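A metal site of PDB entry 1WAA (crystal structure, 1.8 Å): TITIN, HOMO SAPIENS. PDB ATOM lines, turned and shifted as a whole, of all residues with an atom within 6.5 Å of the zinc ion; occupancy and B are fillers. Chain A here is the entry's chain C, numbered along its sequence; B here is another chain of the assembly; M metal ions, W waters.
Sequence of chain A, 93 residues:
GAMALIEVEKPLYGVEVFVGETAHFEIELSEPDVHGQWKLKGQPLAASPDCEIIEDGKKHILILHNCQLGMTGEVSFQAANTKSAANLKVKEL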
ATOM      1  N   THR A  22      31.942  16.879 -23.537  1.00  0.00           N
ATOM      2  CA  THR A  22      31.656  17.516 -22.252  1.00  0.00           C
ATOM      3  C   THR A  22      32.904  18.195 -21.660  1.00  0.00           C
ATOM      4  O   THR A  22      34.051  17.751 -21.827  1.00  0.00           O
ATOM      5  CB  THR A  22      30.929  16.554 -21.230  1.00  0.00           C
ATOM      6  OG1 THR A  22      31.626  16.444 -19.982  1.00  0.00           O
ATOM      7  CG2 THR A  22      30.711  15.169 -21.768  1.00  0.00           C
ATOM      8  N   PRO A  49      20.010  18.332 -17.064  1.00  0.00           N
ATOM      9  CA  PRO A  49      20.745  17.147 -17.456  1.00  0.00           C
ATOM     10  C   PRO A  49      22.111  17.435 -18.088  1.00  0.00           C
ATOM     11  O   PRO A  49      23.072  16.655 -17.855  1.00  0.00           O
ATOM     12  CB  PRO A  49      19.793  16.410 -18.374  1.00  0.00           C
ATOM     13  CG  PRO A  49      18.441  17.042 -18.198  1.00  0.00           C
ATOM     14  CD  PRO A  49      18.646  18.396 -17.609  1.00  0.00           C
ATOM     15  N   GLU A  52      25.495  20.075 -14.731  1.00  0.00           N
ATOM     16  CA  GLU A  52      25.546  19.465 -13.412  1.00  0.00           C
ATOM     17  C   GLU A  52      26.521  20.214 -12.508  1.00  0.00           C
ATOM     18  O   GLU A  52      27.661  20.494 -12.881  1.00  0.00           O
ATOM     19  CB  GLU A  52      25.919  17.983 -13.585  1.00  0.00           C
ATOM     20  CG  GLU A  52      24.997  17.263 -14.591  1.00  0.00           C
ATOM     21  CD  GLU A  52      25.395  15.823 -14.853  1.00  0.00           C
ATOM     22  OE1 GLU A  52      24.518  14.909 -14.757  1.00  0.00           O
ATOM     23  OE2 GLU A  52      26.586  15.548 -15.135  1.00  0.00           O
ATOM     24  N   ILE A  63      29.959  20.363 -14.602  1.00  0.00           N
ATOM     25  CA  ILE A  63      30.017  19.498 -15.776  1.00  0.00           C
ATOM     26  C   ILE A  63      29.027  20.031 -16.792  1.00  0.00           C
ATOM     27  O   ILE A  63      27.822  20.162 -16.502  1.00  0.00           O
ATOM     28  CB  ILE A  63      29.665  18.047 -15.417  1.00  0.00           C
ATOM     29  CG1 ILE A  63      30.621  17.511 -14.327  1.00  0.00           C
ATOM     30  CG2 ILE A  63      29.692  17.152 -16.675  1.00  0.00           C
ATOM     31  CD1 ILE A  63      30.370  16.079 -13.871  1.00  0.00           C
ATOM     32  N   HIS A  65      27.571  19.100 -20.421  1.00  0.00           N
ATOM     33  CA  HIS A  65      27.495  18.092 -21.477  1.00  0.00           C
ATOM     34  C   HIS A  65      27.081  18.720 -22.773  1.00  0.00           C
ATOM     35  O   HIS A  65      26.490  19.781 -22.765  1.00  0.00           O
ATOM     36  CB  HIS A  65      26.452  17.040 -21.121  1.00  0.00           C
ATOM     37  CG  HIS A  65      26.898  16.149 -20.000  1.00  0.00           C
ATOM     38  ND1 HIS A  65      28.002  15.342 -20.108  1.00  0.00           N
ATOM     39  CD2 HIS A  65      26.392  15.951 -18.763  1.00  0.00           C
ATOM     40  CE1 HIS A  65      28.146  14.673 -18.973  1.00  0.00           C
ATOM     41  NE2 HIS A  65      27.186  15.031 -18.149  1.00  0.00           N
ATOM     42  N   LYS B  10      23.983   5.921 -15.298  1.00  0.00           N
ATOM     43  CA  LYS B  10      24.727   6.496 -16.432  1.00  0.00           C
ATOM     44  C   LYS B  10      26.127   5.967 -16.366  1.00  0.00           C
ATOM     45  O   LYS B  10      26.849   6.235 -15.393  1.00  0.00           O
ATOM     46  CB  LYS B  10      24.745   8.031 -16.401  1.00  0.00           C
ATOM     47  CG  LYS B  10      23.356   8.649 -16.325  1.00  0.00           C
ATOM     48  CD  LYS B  10      23.335  10.113 -16.720  1.00  0.00           C
ATOM     49  CE  LYS B  10      21.907  10.659 -16.671  1.00  0.00           C
ATOM     50  NZ  LYS B  10      21.306  10.444 -15.319  1.00  0.00           N
ATOM     51  N   GLU B  26      33.021  10.043 -15.036  1.00  0.00           N
ATOM     52  CA  GLU B  26      31.769  10.318 -14.317  1.00  0.00           C
ATOM     53  C   GLU B  26      30.846   9.131 -14.499  1.00  0.00           C
ATOM     54  O   GLU B  26      30.562   8.683 -15.639  1.00  0.00           O
ATOM     55  CB  GLU B  26      31.145  11.622 -14.833  1.00  0.00           C
ATOM     56  CG  GLU B  26      29.796  12.030 -14.185  1.00  0.00           C
ATOM     57  CD  GLU B  26      28.890  12.761 -15.133  1.00  0.00           C
ATOM     58  OE1 GLU B  26      27.778  13.089 -14.706  1.00  0.00           O
ATOM     59  OE2 GLU B  26      29.255  12.961 -16.307  1.00  0.00           O
ATOM     60  N   LYS B  59      26.393  10.549  -7.772  1.00  0.00           N
ATOM     61  CA  LYS B  59      27.473  10.692  -8.760  1.00  0.00           C
ATOM     62  C   LYS B  59      28.862  10.432  -8.202  1.00  0.00           C
ATOM     63  O   LYS B  59      29.198  10.874  -7.104  1.00  0.00           O
ATOM     64  CB  LYS B  59      27.502  12.088  -9.347  1.00  0.00           C
ATOM     65  CG  LYS B  59      26.264  12.536  -9.988  1.00  0.00           C
ATOM     66  CD  LYS B  59      26.449  13.922 -10.573  1.00  0.00           C
ATOM     67  CE  LYS B  59      26.724  13.822 -12.031  1.00  0.00           C
ATOM     68  NZ  LYS B  59      25.671  12.974 -12.668  1.00  0.00           N
HETATM   69 ZN    ZN M   1      26.939  14.081 -16.279  1.00  0.00          ZN
HETATM   70  O   HOH W   1      25.397  12.664 -16.749  1.00  0.00           O
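Lys 59 of chain B touches the zinc ion (NZ to ZN, 3.98 Å). Of the 8 residues printed, 4 come within 4 Å of the zinc ion.
OE1 of Glu 52 is in salt-bridge range of NZ of Lys 59 of chain B (3.1 Å). The backbone carbonyl oxygen of Glu 52 lies within hydrogen-bond range of the backbone NH of Ile 63 (2.9 Å). OE1 of Glu 26 of chain B sits close to NZ of Lys 59 of chain B.
OE2 of Glu 52 binds the zinc ion, 1.9 Å away. The zinc ion is bound by OE1 of Glu 26 of chain B, at 2.0 Å. The zinc ion is bound by a ring nitrogen (NE2) of His 65, 2.1 Å away. The zinc ion is bound by water W1, 2.1 Å away. The side-chain carboxylate (OE2) of Glu 26 of chain B binds the zinc ion (2.6 Å).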
